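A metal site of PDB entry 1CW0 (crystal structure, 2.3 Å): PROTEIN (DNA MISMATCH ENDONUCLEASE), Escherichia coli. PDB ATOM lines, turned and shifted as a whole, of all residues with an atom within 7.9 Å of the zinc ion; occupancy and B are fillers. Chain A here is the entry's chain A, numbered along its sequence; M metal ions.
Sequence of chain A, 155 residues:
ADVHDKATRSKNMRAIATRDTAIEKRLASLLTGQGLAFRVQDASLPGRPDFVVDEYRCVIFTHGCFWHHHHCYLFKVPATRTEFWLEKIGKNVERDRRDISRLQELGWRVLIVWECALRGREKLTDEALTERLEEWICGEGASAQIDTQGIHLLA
N of Cys 65 is in hydrogen-bond range of OE1 of Glu 115, 2.9 Å away.
N of Leu 74 sits close to SG of Cys 72, 3.3 Å away.
Of the 20 residues printed, 4 come within 4 Å of the zinc ion.
The nearest printed residue that does not touch the zinc ion is Trp 114 (4.4 Å).
The zinc ion is bound by a ring nitrogen (ND1) of His 70 (1.9 Å), the side-chain sulfur (SG) of Cys 65 (2.3 Å), the side-chain sulfur (SG) of Cys 72 (2.4 Å) and the side-chain sulfur (SG) of Cys 116 (2.4 Å).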
ATOM      1  N   HIS A  63       6.208  21.471 -29.857  1.00  0.00           N
ATOM      2  CA  HIS A  63       7.509  21.642 -30.496  1.00  0.00           C
ATOM      3  C   HIS A  63       8.218  20.340 -30.831  1.00  0.00           C
ATOM      4  O   HIS A  63       8.517  19.536 -29.950  1.00  0.00           O
ATOM      5  CB  HIS A  63       8.443  22.451 -29.585  1.00  0.00           C
ATOM      6  CG  HIS A  63       8.271  23.935 -29.663  1.00  0.00           C
ATOM      7  ND1 HIS A  63       7.291  24.554 -30.399  1.00  0.00           N
ATOM      8  CD2 HIS A  63       8.979  24.932 -29.062  1.00  0.00           C
ATOM      9  CE1 HIS A  63       7.392  25.864 -30.259  1.00  0.00           C
ATOM     10  NE2 HIS A  63       8.411  26.111 -29.456  1.00  0.00           N
ATOM     11  N   GLY A  64       8.589  20.204 -32.108  1.00  0.00           N
ATOM     12  CA  GLY A  64       9.388  19.063 -32.498  1.00  0.00           C
ATOM     13  C   GLY A  64      10.782  19.303 -31.931  1.00  0.00           C
ATOM     14  O   GLY A  64      11.303  20.422 -32.054  1.00  0.00           O
ATOM     15  N   CYS A  65      11.339  18.325 -31.243  1.00  0.00           N
ATOM     16  CA  CYS A  65      12.640  18.515 -30.584  1.00  0.00           C
ATOM     17  C   CYS A  65      13.810  18.831 -31.520  1.00  0.00           C
ATOM     18  O   CYS A  65      14.712  19.567 -31.137  1.00  0.00           O
ATOM     19  CB  CYS A  65      12.918  17.442 -29.535  1.00  0.00           C
ATOM     20  SG  CYS A  65      11.554  17.318 -28.319  1.00  0.00           S
ATOM     21  N   PHE A  66      13.767  18.327 -32.746  1.00  0.00           N
ATOM     22  CA  PHE A  66      14.820  18.649 -33.718  1.00  0.00           C
ATOM     23  C   PHE A  66      14.648  20.088 -34.243  1.00  0.00           C
ATOM     24  O   PHE A  66      15.552  20.920 -34.114  1.00  0.00           O
ATOM     25  CB  PHE A  66      14.754  17.658 -34.897  1.00  0.00           C
ATOM     26  CG  PHE A  66      15.656  17.970 -36.063  1.00  0.00           C
ATOM     27  CD1 PHE A  66      17.039  17.968 -35.925  1.00  0.00           C
ATOM     28  CD2 PHE A  66      15.112  18.253 -37.311  1.00  0.00           C
ATOM     29  CE1 PHE A  66      17.865  18.235 -36.997  1.00  0.00           C
ATOM     30  CE2 PHE A  66      15.933  18.522 -38.400  1.00  0.00           C
ATOM     31  CZ  PHE A  66      17.315  18.514 -38.238  1.00  0.00           C
ATOM     32  N   HIS A  69      15.109  22.679 -31.614  1.00  0.00           N
ATOM     33  CA  HIS A  69      16.298  22.451 -30.808  1.00  0.00           C
ATOM     34  C   HIS A  69      16.029  22.291 -29.318  1.00  0.00           C
ATOM     35  O   HIS A  69      16.456  23.132 -28.512  1.00  0.00           O
ATOM     36  CB  HIS A  69      17.392  23.494 -31.055  1.00  0.00           C
ATOM     37  CG  HIS A  69      18.691  23.126 -30.379  1.00  0.00           C
ATOM     38  ND1 HIS A  69      19.799  23.943 -30.380  1.00  0.00           N
ATOM     39  CD2 HIS A  69      19.047  22.003 -29.703  1.00  0.00           C
ATOM     40  CE1 HIS A  69      20.782  23.344 -29.715  1.00  0.00           C
ATOM     41  NE2 HIS A  69      20.350  22.175 -29.298  1.00  0.00           N
ATOM     42  N   HIS A  70      15.422  21.188 -28.941  1.00  0.00           N
ATOM     43  CA  HIS A  70      15.239  20.914 -27.533  1.00  0.00           C
ATOM     44  C   HIS A  70      16.569  20.297 -27.091  1.00  0.00           C
ATOM     45  O   HIS A  70      17.180  19.558 -27.876  1.00  0.00           O
ATOM     46  CB  HIS A  70      14.126  19.887 -27.309  1.00  0.00           C
ATOM     47  CG  HIS A  70      13.615  19.792 -25.900  1.00  0.00           C
ATOM     48  ND1 HIS A  70      12.994  18.643 -25.447  1.00  0.00           N
ATOM     49  CD2 HIS A  70      13.595  20.734 -24.923  1.00  0.00           C
ATOM     50  CE1 HIS A  70      12.601  18.908 -24.221  1.00  0.00           C
ATOM     51  NE2 HIS A  70      12.937  20.166 -23.849  1.00  0.00           N
ATOM     52  N   HIS A  71      17.021  20.576 -25.892  1.00  0.00           N
ATOM     53  CA  HIS A  71      18.279  19.974 -25.445  1.00  0.00           C
ATOM     54  C   HIS A  71      17.991  18.628 -24.765  1.00  0.00           C
ATOM     55  O   HIS A  71      18.089  18.483 -23.548  1.00  0.00           O
ATOM     56  CB  HIS A  71      19.077  20.921 -24.549  1.00  0.00           C
ATOM     57  CG  HIS A  71      19.525  22.158 -25.277  1.00  0.00           C
ATOM     58  ND1 HIS A  71      20.836  22.593 -25.300  1.00  0.00           N
ATOM     59  CD2 HIS A  71      18.823  23.049 -26.027  1.00  0.00           C
ATOM     60  CE1 HIS A  71      20.923  23.696 -26.027  1.00  0.00           C
ATOM     61  NE2 HIS A  71      19.720  23.990 -26.482  1.00  0.00           N
ATOM     62  N   CYS A  72      17.556  17.680 -25.575  1.00  0.00           N
ATOM     63  CA  CYS A  72      17.169  16.355 -25.088  1.00  0.00           C
ATOM     64  C   CYS A  72      17.750  15.272 -25.982  1.00  0.00           C
ATOM     65  O   CYS A  72      18.366  15.562 -26.993  1.00  0.00           O
ATOM     66  CB  CYS A  72      15.638  16.259 -25.063  1.00  0.00           C
ATOM     67  SG  CYS A  72      14.880  16.028 -26.706  1.00  0.00           S
ATOM     68  N   TYR A  73      17.537  14.018 -25.609  1.00  0.00           N
ATOM     69  CA  TYR A  73      18.054  12.865 -26.356  1.00  0.00           C
ATOM     70  C   TYR A  73      17.560  12.806 -27.811  1.00  0.00           C
ATOM     71  O   TYR A  73      18.144  12.098 -28.631  1.00  0.00           O
ATOM     72  CB  TYR A  73      17.734  11.551 -25.631  1.00  0.00           C
ATOM     73  CG  TYR A  73      16.336  11.033 -25.882  1.00  0.00           C
ATOM     74  CD1 TYR A  73      16.079  10.072 -26.858  1.00  0.00           C
ATOM     75  CD2 TYR A  73      15.262  11.514 -25.141  1.00  0.00           C
ATOM     76  CE1 TYR A  73      14.801   9.611 -27.081  1.00  0.00           C
ATOM     77  CE2 TYR A  73      13.971  11.056 -25.360  1.00  0.00           C
ATOM     78  CZ  TYR A  73      13.751  10.111 -26.326  1.00  0.00           C
ATOM     79  OH  TYR A  73      12.472   9.670 -26.539  1.00  0.00           O
ATOM     80  N   LEU A  74      16.489  13.510 -28.127  1.00  0.00           N
ATOM     81  CA  LEU A  74      15.970  13.471 -29.510  1.00  0.00           C
ATOM     82  C   LEU A  74      16.769  14.373 -30.461  1.00  0.00           C
ATOM     83  O   LEU A  74      16.656  14.227 -31.679  1.00  0.00           O
ATOM     84  CB  LEU A  74      14.485  13.851 -29.548  1.00  0.00           C
ATOM     85  CG  LEU A  74      13.479  12.791 -29.074  1.00  0.00           C
ATOM     86  CD1 LEU A  74      12.054  13.310 -29.174  1.00  0.00           C
ATOM     87  CD2 LEU A  74      13.647  11.490 -29.844  1.00  0.00           C
ATOM     88  N   PHE A  75      17.529  15.329 -29.907  1.00  0.00           N
ATOM     89  CA  PHE A  75      18.273  16.273 -30.730  1.00  0.00           C
ATOM     90  C   PHE A  75      19.753  15.949 -30.944  1.00  0.00           C
ATOM     91  O   PHE A  75      20.538  15.791 -30.005  1.00  0.00           O
ATOM     92  CB  PHE A  75      18.145  17.696 -30.184  1.00  0.00           C
ATOM     93  CG  PHE A  75      18.859  18.701 -31.043  1.00  0.00           C
ATOM     94  CD1 PHE A  75      18.181  19.355 -32.055  1.00  0.00           C
ATOM     95  CD2 PHE A  75      20.206  18.955 -30.852  1.00  0.00           C
ATOM     96  CE1 PHE A  75      18.845  20.259 -32.867  1.00  0.00           C
ATOM     97  CE2 PHE A  75      20.869  19.859 -31.664  1.00  0.00           C
ATOM     98  CZ  PHE A  75      20.193  20.502 -32.665  1.00  0.00           C
ATOM     99  N   VAL A 113       4.642  22.418 -25.457  1.00  0.00           N
ATOM    100  CA  VAL A 113       4.640  20.989 -25.232  1.00  0.00           C
ATOM    101  C   VAL A 113       5.691  20.360 -26.131  1.00  0.00           C
ATOM    102  O   VAL A 113       5.523  20.311 -27.347  1.00  0.00           O
ATOM    103  CB  VAL A 113       3.249  20.331 -25.490  1.00  0.00           C
ATOM    104  CG1 VAL A 113       3.298  18.837 -25.188  1.00  0.00           C
ATOM    105  CG2 VAL A 113       2.179  21.002 -24.627  1.00  0.00           C
ATOM    106  N   TRP A 114       6.794  19.903 -25.533  1.00  0.00           N
ATOM    107  CA  TRP A 114       7.882  19.312 -26.302  1.00  0.00           C
ATOM    108  C   TRP A 114       7.523  17.920 -26.800  1.00  0.00           C
ATOM    109  O   TRP A 114       6.801  17.167 -26.141  1.00  0.00           O
ATOM    110  CB  TRP A 114       9.201  19.329 -25.507  1.00  0.00           C
ATOM    111  CG  TRP A 114       9.738  20.726 -25.275  1.00  0.00           C
ATOM    112  CD1 TRP A 114       9.569  21.492 -24.161  1.00  0.00           C
ATOM    113  CD2 TRP A 114      10.536  21.519 -26.183  1.00  0.00           C
ATOM    114  NE1 TRP A 114      10.195  22.724 -24.309  1.00  0.00           N
ATOM    115  CE2 TRP A 114      10.795  22.757 -25.553  1.00  0.00           C
ATOM    116  CE3 TRP A 114      11.039  21.292 -27.466  1.00  0.00           C
ATOM    117  CZ2 TRP A 114      11.541  23.760 -26.153  1.00  0.00           C
ATOM    118  CZ3 TRP A 114      11.778  22.301 -28.070  1.00  0.00           C
ATOM    119  CH2 TRP A 114      12.023  23.516 -27.421  1.00  0.00           C
ATOM    120  N   GLU A 115       8.011  17.601 -28.003  1.00  0.00           N
ATOM    121  CA  GLU A 115       7.732  16.331 -28.651  1.00  0.00           C
ATOM    122  C   GLU A 115       8.087  15.105 -27.779  1.00  0.00           C
ATOM    123  O   GLU A 115       7.328  14.145 -27.717  1.00  0.00           O
ATOM    124  CB  GLU A 115       8.434  16.271 -30.009  1.00  0.00           C
ATOM    125  CG  GLU A 115       8.618  14.855 -30.546  1.00  0.00           C
ATOM    126  CD  GLU A 115       9.434  14.807 -31.821  1.00  0.00           C
ATOM    127  OE1 GLU A 115      10.252  15.707 -32.057  1.00  0.00           O
ATOM    128  OE2 GLU A 115       9.245  13.843 -32.591  1.00  0.00           O
ATOM    129  N   CYS A 116       9.252  15.130 -27.131  1.00  0.00           N
ATOM    130  CA  CYS A 116       9.682  14.005 -26.301  1.00  0.00           C
ATOM    131  C   CYS A 116       8.650  13.646 -25.219  1.00  0.00           C
ATOM    132  O   CYS A 116       8.585  12.486 -24.777  1.00  0.00           O
ATOM    133  CB  CYS A 116      11.058  14.234 -25.713  1.00  0.00           C
ATOM    134  SG  CYS A 116      11.254  15.828 -24.851  1.00  0.00           S
ATOM    135  N   ALA A 117       7.833  14.616 -24.803  1.00  0.00           N
ATOM    136  CA  ALA A 117       6.803  14.354 -23.797  1.00  0.00           C
ATOM    137  C   ALA A 117       5.576  13.675 -24.415  1.00  0.00           C
ATOM    138  O   ALA A 117       4.792  13.029 -23.712  1.00  0.00           O
ATOM    139  CB  ALA A 117       6.398  15.650 -23.097  1.00  0.00           C
ATOM    140  N   ARG A 119       5.849  11.723 -27.598  1.00  0.00           N
ATOM    141  CA  ARG A 119       6.191  10.441 -28.246  1.00  0.00           C
ATOM    142  C   ARG A 119       7.619  10.027 -27.928  1.00  0.00           C
ATOM    143  O   ARG A 119       8.454  10.859 -27.552  1.00  0.00           O
ATOM    144  CB  ARG A 119       6.011  10.448 -29.760  1.00  0.00           C
ATOM    145  CG  ARG A 119       6.451  11.712 -30.481  1.00  0.00           C
ATOM    146  CD  ARG A 119       7.660  11.446 -31.379  1.00  0.00           C
ATOM    147  NE  ARG A 119       7.734  10.052 -31.831  1.00  0.00           N
ATOM    148  CZ  ARG A 119       7.924   9.668 -33.113  1.00  0.00           C
ATOM    149  NH1 ARG A 119       7.607  10.476 -34.116  1.00  0.00           N
ATOM    150  NH2 ARG A 119       8.426   8.463 -33.375  1.00  0.00           N
ATOM    151  N   ILE A 146       6.181  21.694 -21.028  1.00  0.00           N
ATOM    152  CA  ILE A 146       6.101  20.329 -20.573  1.00  0.00           C
ATOM    153  C   ILE A 146       7.097  19.480 -21.322  1.00  0.00           C
ATOM    154  O   ILE A 146       7.039  19.380 -22.543  1.00  0.00           O
ATOM    155  CB  ILE A 146       4.703  19.718 -20.816  1.00  0.00           C
ATOM    156  CG1 ILE A 146       3.627  20.454 -20.007  1.00  0.00           C
ATOM    157  CG2 ILE A 146       4.727  18.230 -20.474  1.00  0.00           C
ATOM    158  CD1 ILE A 146       2.230  20.063 -20.402  1.00  0.00           C
ATOM    159  N   ASP A 147       7.980  18.836 -20.566  1.00  0.00           N
ATOM    160  CA  ASP A 147       8.962  17.943 -21.129  1.00  0.00           C
ATOM    161  C   ASP A 147       8.802  16.574 -20.480  1.00  0.00           C
ATOM    162  O   ASP A 147       7.758  16.302 -19.874  1.00  0.00           O
ATOM    163  CB  ASP A 147      10.379  18.484 -20.946  1.00  0.00           C
ATOM    164  CG  ASP A 147      10.653  18.970 -19.543  1.00  0.00           C
ATOM    165  OD1 ASP A 147      10.205  18.309 -18.578  1.00  0.00           O
ATOM    166  OD2 ASP A 147      11.329  20.006 -19.402  1.00  0.00           O
ATOM    167  N   THR A 148       9.828  15.715 -20.591  1.00  0.00           N
ATOM    168  CA  THR A 148       9.760  14.383 -19.988  1.00  0.00           C
ATOM    169  C   THR A 148       9.767  14.456 -18.451  1.00  0.00           C
ATOM    170  O   THR A 148       9.366  13.505 -17.781  1.00  0.00           O
ATOM    171  CB  THR A 148      10.881  13.465 -20.505  1.00  0.00           C
ATOM    172  OG1 THR A 148      12.159  14.001 -20.190  1.00  0.00           O
ATOM    173  CG2 THR A 148      10.825  13.193 -21.999  1.00  0.00           C
HETATM  174 ZN    ZN M   1      12.745  16.965 -26.393  1.00  0.00          ZN
